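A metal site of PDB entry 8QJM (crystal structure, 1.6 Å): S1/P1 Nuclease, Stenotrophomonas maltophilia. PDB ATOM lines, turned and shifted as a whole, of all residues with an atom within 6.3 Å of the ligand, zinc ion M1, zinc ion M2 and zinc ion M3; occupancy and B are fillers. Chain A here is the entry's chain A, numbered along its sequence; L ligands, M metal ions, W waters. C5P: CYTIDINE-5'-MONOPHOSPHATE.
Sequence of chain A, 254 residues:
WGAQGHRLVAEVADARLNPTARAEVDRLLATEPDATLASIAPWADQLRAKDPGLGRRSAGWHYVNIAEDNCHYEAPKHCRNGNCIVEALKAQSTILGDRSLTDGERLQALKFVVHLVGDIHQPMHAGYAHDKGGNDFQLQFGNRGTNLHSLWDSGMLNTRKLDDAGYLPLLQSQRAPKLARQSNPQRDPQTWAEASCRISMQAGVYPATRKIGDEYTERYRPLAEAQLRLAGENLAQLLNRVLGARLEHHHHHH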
ATOM      1  N   TRP A   1     -32.193  27.099  19.749  1.00  0.00           N
ATOM      2  CA  TRP A   1     -33.415  27.282  20.626  1.00  0.00           C
ATOM      3  C   TRP A   1     -33.071  28.190  21.802  1.00  0.00           C
ATOM      4  O   TRP A   1     -31.886  28.222  22.224  1.00  0.00           O
ATOM      5  CB  TRP A   1     -33.922  25.928  21.153  1.00  0.00           C
ATOM      6  CG  TRP A   1     -34.200  24.951  20.055  1.00  0.00           C
ATOM      7  CD1 TRP A   1     -33.438  23.858  19.747  1.00  0.00           C
ATOM      8  CD2 TRP A   1     -35.286  24.976  19.139  1.00  0.00           C
ATOM      9  NE1 TRP A   1     -33.989  23.231  18.665  1.00  0.00           N
ATOM     10  CE2 TRP A   1     -35.104  23.900  18.266  1.00  0.00           C
ATOM     11  CE3 TRP A   1     -36.385  25.810  18.925  1.00  0.00           C
ATOM     12  CZ2 TRP A   1     -36.008  23.569  17.258  1.00  0.00           C
ATOM     13  CZ3 TRP A   1     -37.255  25.534  17.906  1.00  0.00           C
ATOM     14  CH2 TRP A   1     -37.073  24.415  17.084  1.00  0.00           C
ATOM     15  N   GLY A   2     -34.109  28.786  22.403  1.00  0.00           N
ATOM     16  CA  GLY A   2     -34.099  29.354  23.750  1.00  0.00           C
ATOM     17  C   GLY A   2     -33.959  28.238  24.766  1.00  0.00           C
ATOM     18  O   GLY A   2     -33.847  27.059  24.399  1.00  0.00           O
ATOM     19  N   ALA A   3     -33.828  28.624  26.015  1.00  0.00           N
ATOM     20  CA  ALA A   3     -33.528  27.711  27.119  1.00  0.00           C
ATOM     21  C   ALA A   3     -34.600  26.620  27.131  1.00  0.00           C
ATOM     22  O   ALA A   3     -34.231  25.452  27.354  1.00  0.00           O
ATOM     23  CB  ALA A   3     -33.499  28.474  28.451  1.00  0.00           C
ATOM     24  N   HIS A   6     -34.112  23.942  24.500  1.00  0.00           N
ATOM     25  CA  HIS A   6     -32.958  23.053  24.826  1.00  0.00           C
ATOM     26  C   HIS A   6     -33.419  22.022  25.849  1.00  0.00           C
ATOM     27  O   HIS A   6     -33.021  20.816  25.748  1.00  0.00           O
ATOM     28  CB  HIS A   6     -31.761  23.925  25.237  1.00  0.00           C
ATOM     29  CG  HIS A   6     -31.106  24.495  24.033  1.00  0.00           C
ATOM     30  ND1 HIS A   6     -30.409  23.707  23.134  1.00  0.00           N
ATOM     31  CD2 HIS A   6     -31.087  25.755  23.514  1.00  0.00           C
ATOM     32  CE1 HIS A   6     -30.000  24.466  22.131  1.00  0.00           C
ATOM     33  NE2 HIS A   6     -30.389  25.688  22.323  1.00  0.00           N
ATOM     34  N   ALA A  44     -24.333  25.684  27.092  1.00  0.00           N
ATOM     35  CA  ALA A  44     -23.401  26.147  26.045  1.00  0.00           C
ATOM     36  C   ALA A  44     -23.725  27.603  25.661  1.00  0.00           C
ATOM     37  O   ALA A  44     -22.754  28.308  25.376  1.00  0.00           O
ATOM     38  CB  ALA A  44     -23.408  25.189  24.876  1.00  0.00           C
ATOM     39  N   ASP A  45     -24.978  28.060  25.728  1.00  0.00           N
ATOM     40  CA  ASP A  45     -25.338  29.481  25.416  1.00  0.00           C
ATOM     41  C   ASP A  45     -24.861  30.392  26.549  1.00  0.00           C
ATOM     42  O   ASP A  45     -24.446  31.532  26.247  1.00  0.00           O
ATOM     43  CB  ASP A  45     -26.837  29.669  25.191  1.00  0.00           C
ATOM     44  CG  ASP A  45     -27.358  28.982  23.962  1.00  0.00           C
ATOM     45  OD1 ASP A  45     -26.582  28.783  23.020  1.00  0.00           O
ATOM     46  OD2 ASP A  45     -28.546  28.624  23.932  1.00  0.00           O
ATOM     47  N   GLN A  46     -24.940  29.935  27.787  1.00  0.00           N
ATOM     48  CA  GLN A  46     -24.475  30.698  28.966  1.00  0.00           C
ATOM     49  C   GLN A  46     -22.943  30.813  28.880  1.00  0.00           C
ATOM     50  O   GLN A  46     -22.438  31.893  29.130  1.00  0.00           O
ATOM     51  CB  GLN A  46     -24.988  30.061  30.255  1.00  0.00           C
ATOM     52  CG  GLN A  46     -26.464  30.316  30.481  1.00  0.00           C
ATOM     53  CD  GLN A  46     -26.837  31.739  30.131  1.00  0.00           C
ATOM     54  OE1 GLN A  46     -26.391  32.680  30.784  1.00  0.00           O
ATOM     55  NE2 GLN A  46     -27.652  31.912  29.116  1.00  0.00           N
ATOM     56  N   ARG A  48     -21.158  30.826  26.157  1.00  0.00           N
ATOM     57  CA  ARG A  48     -20.930  31.843  25.074  1.00  0.00           C
ATOM     58  C   ARG A  48     -21.109  33.261  25.648  1.00  0.00           C
ATOM     59  O   ARG A  48     -20.262  34.173  25.307  1.00  0.00           O
ATOM     60  CB  ARG A  48     -21.826  31.550  23.851  1.00  0.00           C
ATOM     61  CG  ARG A  48     -21.610  32.511  22.687  1.00  0.00           C
ATOM     62  CD  ARG A  48     -22.656  32.360  21.591  1.00  0.00           C
ATOM     63  NE  ARG A  48     -23.956  32.622  22.143  1.00  0.00           N
ATOM     64  CZ  ARG A  48     -25.057  31.915  21.902  1.00  0.00           C
ATOM     65  NH1 ARG A  48     -25.057  30.921  21.017  1.00  0.00           N
ATOM     66  NH2 ARG A  48     -26.174  32.227  22.534  1.00  0.00           N
ATOM     67  N   ALA A  49     -22.129  33.476  26.473  1.00  0.00           N
ATOM     68  CA  ALA A  49     -22.457  34.800  27.052  1.00  0.00           C
ATOM     69  C   ALA A  49     -21.370  35.226  28.034  1.00  0.00           C
ATOM     70  O   ALA A  49     -21.019  36.435  28.028  1.00  0.00           O
ATOM     71  CB  ALA A  49     -23.801  34.791  27.741  1.00  0.00           C
ATOM     72  N   HIS A  62     -22.503  26.814  17.368  1.00  0.00           N
ATOM     73  CA  HIS A  62     -23.967  26.684  17.553  1.00  0.00           C
ATOM     74  C   HIS A  62     -24.693  26.693  16.200  1.00  0.00           C
ATOM     75  O   HIS A  62     -25.879  26.476  16.215  1.00  0.00           O
ATOM     76  CB  HIS A  62     -24.536  27.788  18.450  1.00  0.00           C
ATOM     77  CG  HIS A  62     -23.992  27.776  19.830  1.00  0.00           C
ATOM     78  ND1 HIS A  62     -24.799  27.621  20.954  1.00  0.00           N
ATOM     79  CD2 HIS A  62     -22.708  27.857  20.273  1.00  0.00           C
ATOM     80  CE1 HIS A  62     -24.020  27.676  22.018  1.00  0.00           C
ATOM     81  NE2 HIS A  62     -22.736  27.778  21.641  1.00  0.00           N
ATOM     82  N   HIS A 115     -26.710  20.177  23.947  1.00  0.00           N
ATOM     83  CA  HIS A 115     -27.007  21.518  23.396  1.00  0.00           C
ATOM     84  C   HIS A 115     -27.040  21.451  21.875  1.00  0.00           C
ATOM     85  O   HIS A 115     -27.976  22.068  21.246  1.00  0.00           O
ATOM     86  CB  HIS A 115     -25.972  22.561  23.877  1.00  0.00           C
ATOM     87  CG  HIS A 115     -26.426  23.947  23.497  1.00  0.00           C
ATOM     88  ND1 HIS A 115     -27.327  24.692  24.257  1.00  0.00           N
ATOM     89  CD2 HIS A 115     -26.154  24.670  22.397  1.00  0.00           C
ATOM     90  CE1 HIS A 115     -27.549  25.858  23.632  1.00  0.00           C
ATOM     91  NE2 HIS A 115     -26.855  25.847  22.474  1.00  0.00           N
ATOM     92  N   LEU A 116     -26.003  20.881  21.248  1.00  0.00           N
ATOM     93  CA  LEU A 116     -25.818  21.012  19.797  1.00  0.00           C
ATOM     94  C   LEU A 116     -26.793  20.155  19.020  1.00  0.00           C
ATOM     95  O   LEU A 116     -27.198  20.574  17.937  1.00  0.00           O
ATOM     96  CB  LEU A 116     -24.370  20.702  19.442  1.00  0.00           C
ATOM     97  CG  LEU A 116     -23.367  21.691  20.000  1.00  0.00           C
ATOM     98  CD1 LEU A 116     -21.938  21.246  19.647  1.00  0.00           C
ATOM     99  CD2 LEU A 116     -23.654  23.119  19.534  1.00  0.00           C
ATOM    100  N   GLY A 118     -29.810  19.835  19.978  1.00  0.00           N
ATOM    101  CA  GLY A 118     -30.868  20.866  19.935  1.00  0.00           C
ATOM    102  C   GLY A 118     -30.681  21.903  18.829  1.00  0.00           C
ATOM    103  O   GLY A 118     -31.555  22.075  17.919  1.00  0.00           O
ATOM    104  N   ASP A 119     -29.584  22.657  18.857  1.00  0.00           N
ATOM    105  CA  ASP A 119     -29.414  23.801  17.916  1.00  0.00           C
ATOM    106  C   ASP A 119     -29.450  23.313  16.454  1.00  0.00           C
ATOM    107  O   ASP A 119     -29.927  24.085  15.598  1.00  0.00           O
ATOM    108  CB  ASP A 119     -28.119  24.550  18.236  1.00  0.00           C
ATOM    109  CG  ASP A 119     -28.292  25.626  19.288  1.00  0.00           C
ATOM    110  OD1 ASP A 119     -29.454  25.910  19.598  1.00  0.00           O
ATOM    111  OD2 ASP A 119     -27.270  26.221  19.730  1.00  0.00           O
ATOM    112  N   GLN A 122     -32.772  23.383  14.864  1.00  0.00           N
ATOM    113  CA  GLN A 122     -33.448  24.712  14.719  1.00  0.00           C
ATOM    114  C   GLN A 122     -33.131  25.188  13.313  1.00  0.00           C
ATOM    115  O   GLN A 122     -31.969  25.467  13.002  1.00  0.00           O
ATOM    116  CB  GLN A 122     -32.946  25.624  15.832  1.00  0.00           C
ATOM    117  CG  GLN A 122     -33.951  26.710  16.264  1.00  0.00           C
ATOM    118  CD  GLN A 122     -34.177  27.779  15.232  1.00  0.00           C
ATOM    119  OE1 GLN A 122     -34.527  27.499  14.086  1.00  0.00           O
ATOM    120  NE2 GLN A 122     -33.985  29.030  15.635  1.00  0.00           N
ATOM    121  N   HIS A 125     -30.581  27.823  12.469  1.00  0.00           N
ATOM    122  CA  HIS A 125     -29.167  27.551  12.825  1.00  0.00           C
ATOM    123  C   HIS A 125     -28.459  26.900  11.626  1.00  0.00           C
ATOM    124  O   HIS A 125     -27.274  26.580  11.767  1.00  0.00           O
ATOM    125  CB  HIS A 125     -29.139  26.650  14.069  1.00  0.00           C
ATOM    126  CG  HIS A 125     -29.340  27.427  15.323  1.00  0.00           C
ATOM    127  ND1 HIS A 125     -28.322  27.517  16.258  1.00  0.00           N
ATOM    128  CD2 HIS A 125     -30.356  28.184  15.817  1.00  0.00           C
ATOM    129  CE1 HIS A 125     -28.696  28.289  17.259  1.00  0.00           C
ATOM    130  NE2 HIS A 125     -29.950  28.660  17.054  1.00  0.00           N
ATOM    131  N   ASN A 135     -30.840  36.361  12.370  1.00  0.00           N
ATOM    132  CA  ASN A 135     -30.633  37.302  13.498  1.00  0.00           C
ATOM    133  C   ASN A 135     -30.785  38.727  12.957  1.00  0.00           C
ATOM    134  O   ASN A 135     -31.336  39.560  13.681  1.00  0.00           O
ATOM    135  CB  ASN A 135     -29.306  37.077  14.228  1.00  0.00           C
ATOM    136  CG  ASN A 135     -29.382  35.948  15.232  1.00  0.00           C
ATOM    137  OD1 ASN A 135     -30.073  36.058  16.239  1.00  0.00           O
ATOM    138  ND2 ASN A 135     -28.665  34.863  14.947  1.00  0.00           N
ATOM    139  N   ASN A 147     -36.737  39.268  15.585  1.00  0.00           N
ATOM    140  CA  ASN A 147     -36.004  38.855  14.370  1.00  0.00           C
ATOM    141  C   ASN A 147     -36.418  37.417  14.101  1.00  0.00           C
ATOM    142  O   ASN A 147     -36.930  36.809  15.062  1.00  0.00           O
ATOM    143  CB  ASN A 147     -34.502  39.076  14.529  1.00  0.00           C
ATOM    144  CG  ASN A 147     -33.888  38.217  15.605  1.00  0.00           C
ATOM    145  OD1 ASN A 147     -33.752  37.020  15.427  1.00  0.00           O
ATOM    146  ND2 ASN A 147     -33.502  38.831  16.701  1.00  0.00           N
ATOM    147  N   HIS A 149     -34.682  34.718  13.588  1.00  0.00           N
ATOM    148  CA  HIS A 149     -33.928  33.775  14.463  1.00  0.00           C
ATOM    149  C   HIS A 149     -34.628  33.593  15.826  1.00  0.00           C
ATOM    150  O   HIS A 149     -34.878  32.411  16.222  1.00  0.00           O
ATOM    151  CB  HIS A 149     -32.475  34.260  14.647  1.00  0.00           C
ATOM    152  CG  HIS A 149     -31.643  33.177  15.216  1.00  0.00           C
ATOM    153  ND1 HIS A 149     -30.935  32.304  14.417  1.00  0.00           N
ATOM    154  CD2 HIS A 149     -31.574  32.738  16.488  1.00  0.00           C
ATOM    155  CE1 HIS A 149     -30.362  31.392  15.206  1.00  0.00           C
ATOM    156  NE2 HIS A 149     -30.782  31.643  16.514  1.00  0.00           N
ATOM    157  N   SER A 150     -34.884  34.685  16.548  1.00  0.00           N
ATOM    158  CA  SER A 150     -35.511  34.675  17.893  1.00  0.00           C
ATOM    159  C   SER A 150     -36.911  34.059  17.795  1.00  0.00           C
ATOM    160  O   SER A 150     -37.349  33.409  18.741  1.00  0.00           O
ATOM    161  CB  SER A 150     -35.596  36.086  18.460  1.00  0.00           C
ATOM    162  OG  SER A 150     -34.284  36.567  18.819  1.00  0.00           O
ATOM    163  N   ASP A 153     -36.155  30.397  17.624  1.00  0.00           N
ATOM    164  CA  ASP A 153     -35.537  29.962  18.919  1.00  0.00           C
ATOM    165  C   ASP A 153     -36.615  29.885  20.018  1.00  0.00           C
ATOM    166  O   ASP A 153     -36.559  28.904  20.797  1.00  0.00           O
ATOM    167  CB  ASP A 153     -34.391  30.881  19.348  1.00  0.00           C
ATOM    168  CG  ASP A 153     -32.999  30.502  18.876  1.00  0.00           C
ATOM    169  OD1 ASP A 153     -32.835  29.477  18.212  1.00  0.00           O
ATOM    170  OD2 ASP A 153     -32.092  31.252  19.182  1.00  0.00           O
HETATM  171  O3P C5P L   1     -28.983  30.771  19.007  1.00  0.00           O
HETATM  172  P   C5P L   1     -28.699  29.862  20.340  1.00  0.00           P
HETATM  173  O1P C5P L   1     -27.275  29.251  20.357  1.00  0.00           O
HETATM  174  O2P C5P L   1     -29.877  28.969  20.410  1.00  0.00           O
HETATM  175  O5' C5P L   1     -28.737  30.876  21.641  1.00  0.00           O
HETATM  176  C5' C5P L   1     -30.020  31.219  22.171  1.00  0.00           C
HETATM  177  C4' C5P L   1     -29.795  31.925  23.472  1.00  0.00           C
HETATM  178  O4' C5P L   1     -29.041  33.134  23.216  1.00  0.00           O
HETATM  179  C3' C5P L   1     -31.046  32.416  24.196  1.00  0.00           C
HETATM  180  O3' C5P L   1     -31.543  31.395  25.057  1.00  0.00           O
HETATM  181  C2' C5P L   1     -30.497  33.570  25.050  1.00  0.00           C
HETATM  182  O2' C5P L   1     -29.818  33.122  26.210  1.00  0.00           O
HETATM  183  C1' C5P L   1     -29.329  34.102  24.212  1.00  0.00           C
HETATM  184  N1  C5P L   1     -29.643  35.394  23.569  1.00  0.00           N
HETATM  185  C2  C5P L   1     -29.553  36.550  24.358  1.00  0.00           C
HETATM  186  N3  C5P L   1     -29.876  37.744  23.814  1.00  0.00           N
HETATM  187  C4  C5P L   1     -30.274  37.837  22.540  1.00  0.00           C
HETATM  188  C5  C5P L   1     -30.387  36.682  21.716  1.00  0.00           C
HETATM  189  C6  C5P L   1     -30.064  35.488  22.260  1.00  0.00           C
HETATM  190  O2  C5P L   1     -29.159  36.450  25.527  1.00  0.00           O
HETATM  191  N4  C5P L   1     -30.585  39.044  22.065  1.00  0.00           N
HETATM  192 ZN    ZN M   1     -26.791  27.484  21.270  1.00  0.00          ZN
HETATM  193 ZN    ZN M   2     -30.436  27.140  21.023  1.00  0.00          ZN
HETATM  194 ZN    ZN M   3     -30.550  30.307  18.040  1.00  0.00          ZN
HETATM  195  O   HOH W   1     -31.882  35.497  19.140  1.00  0.00           O
HETATM  196  O   HOH W   2     -31.452  32.076  28.104  1.00  0.00           O
HETATM  197  O   HOH W   3     -32.514  33.578  20.653  1.00  0.00           O
HETATM  198  O   HOH W   4     -30.426  28.842  25.832  1.00  0.00           O
HETATM  199  O   HOH W   5     -26.322  30.866  17.300  1.00  0.00           O
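A ring nitrogen (ND1) of His 6 lies close to a ring nitrogen (ND1) of His 115 (3.4 Å).
The side-chain amide oxygen (OD1) of Asn 147 sits at hydrogen-bond distance from the backbone NH (N) of His 149 (3.1 Å).
N of Gly 2 lies within hydrogen-bond range of O of Asp 153 (2.9 Å).
ND1 of His 149 lies close to ND2 of Asn 135, at 3.5 Å.
A ring nitrogen (ND1) of His 125 sits at hydrogen-bond distance from the backbone carbonyl oxygen of His 62.
The side-chain amide nitrogen of Gln 122 lies close to the backbone NH of Asp 153 (3.2 Å).
A ring nitrogen (ND1) of His 62 sits close to the guanidinium group of Arg 48.
OD1 of Asp 45 lies close to NH1 of Arg 48 (3.3 Å).
Water W4 lies within hydrogen-bond range of the side-chain carboxylate (OD2) of Asp 45 (2.7 Å), an oxygen (O3') of the ligand (2.9 Å) and the backbone NH (N) of Ala 3 (3.4 Å).
Water W1 bridges the side-chain hydroxyl (OG) of Ser 150 (2.6 Å) and the side-chain amide oxygen (OD1) of Asn 135 (3.5 Å).
Zinc ion M2 is bound by NE2 of His 6, O2P of the ligand, OD1 of Asp 119, N of Trp 1 and O of Trp 1.
The guanidinium group (NH2) of Arg 48 is in hydrogen-bond range of an oxygen (O5') of the ligand (3.0 Å).
Zinc ion M1 is bound by ND1 of His 62 (2.0 Å), NE2 of His 115 (2.0 Å), O1P of the ligand (2.0 Å), OD2 of Asp 119 (2.0 Å) and OD1 of Asp 45 (2.2 Å).
Within 4 Å of zinc ion M3: Trp 1, His 125, His 149 and Asp 153.
The nearest printed residue that does not touch zinc ion M3 is Gln 122 (4.4 Å).
Of the 21 residues printed, 4 come within 4 Å of zinc ion M2.
Along chain A the residues within 4 Å of zinc ion M2 span positions 1 to 119.
Zinc ion M3 is bound by O3P of the ligand, NE2 of His 125, NE2 of His 149, OD2 of Asp 153 and OD1 of Asp 153.
Zinc ion M3 has five donor atoms within binding distance.
Slightly farther from zinc ion M3 lies O2P of the ligand (2.8 Å).
CA of Gly 2 touches O3' of the ligand, at 3.5 Å.
Ala 3 touches the ligand (N to O3', 3.7 Å).
NE2 of Gln 46 touches O2' of the ligand, at 3.8 Å.
Within 4 Å of the ligand: Trp 1, Gly 2, Ala 3, His 6, Asp 45, Gln 46, Arg 48, His 62, Asp 119, His 125, His 149 and Asp 153.
Residues that only touch zinc ion M1: Arg 48.
Within 4 Å of zinc ion M1: Asp 45, Arg 48, His 62, His 115 and Asp 119.
Along chain A the residues within 4 Å of zinc ion M1 span positions 45 to 119.
The nearest printed residue that does not touch zinc ion M1 is His 6 (4.2 Å).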
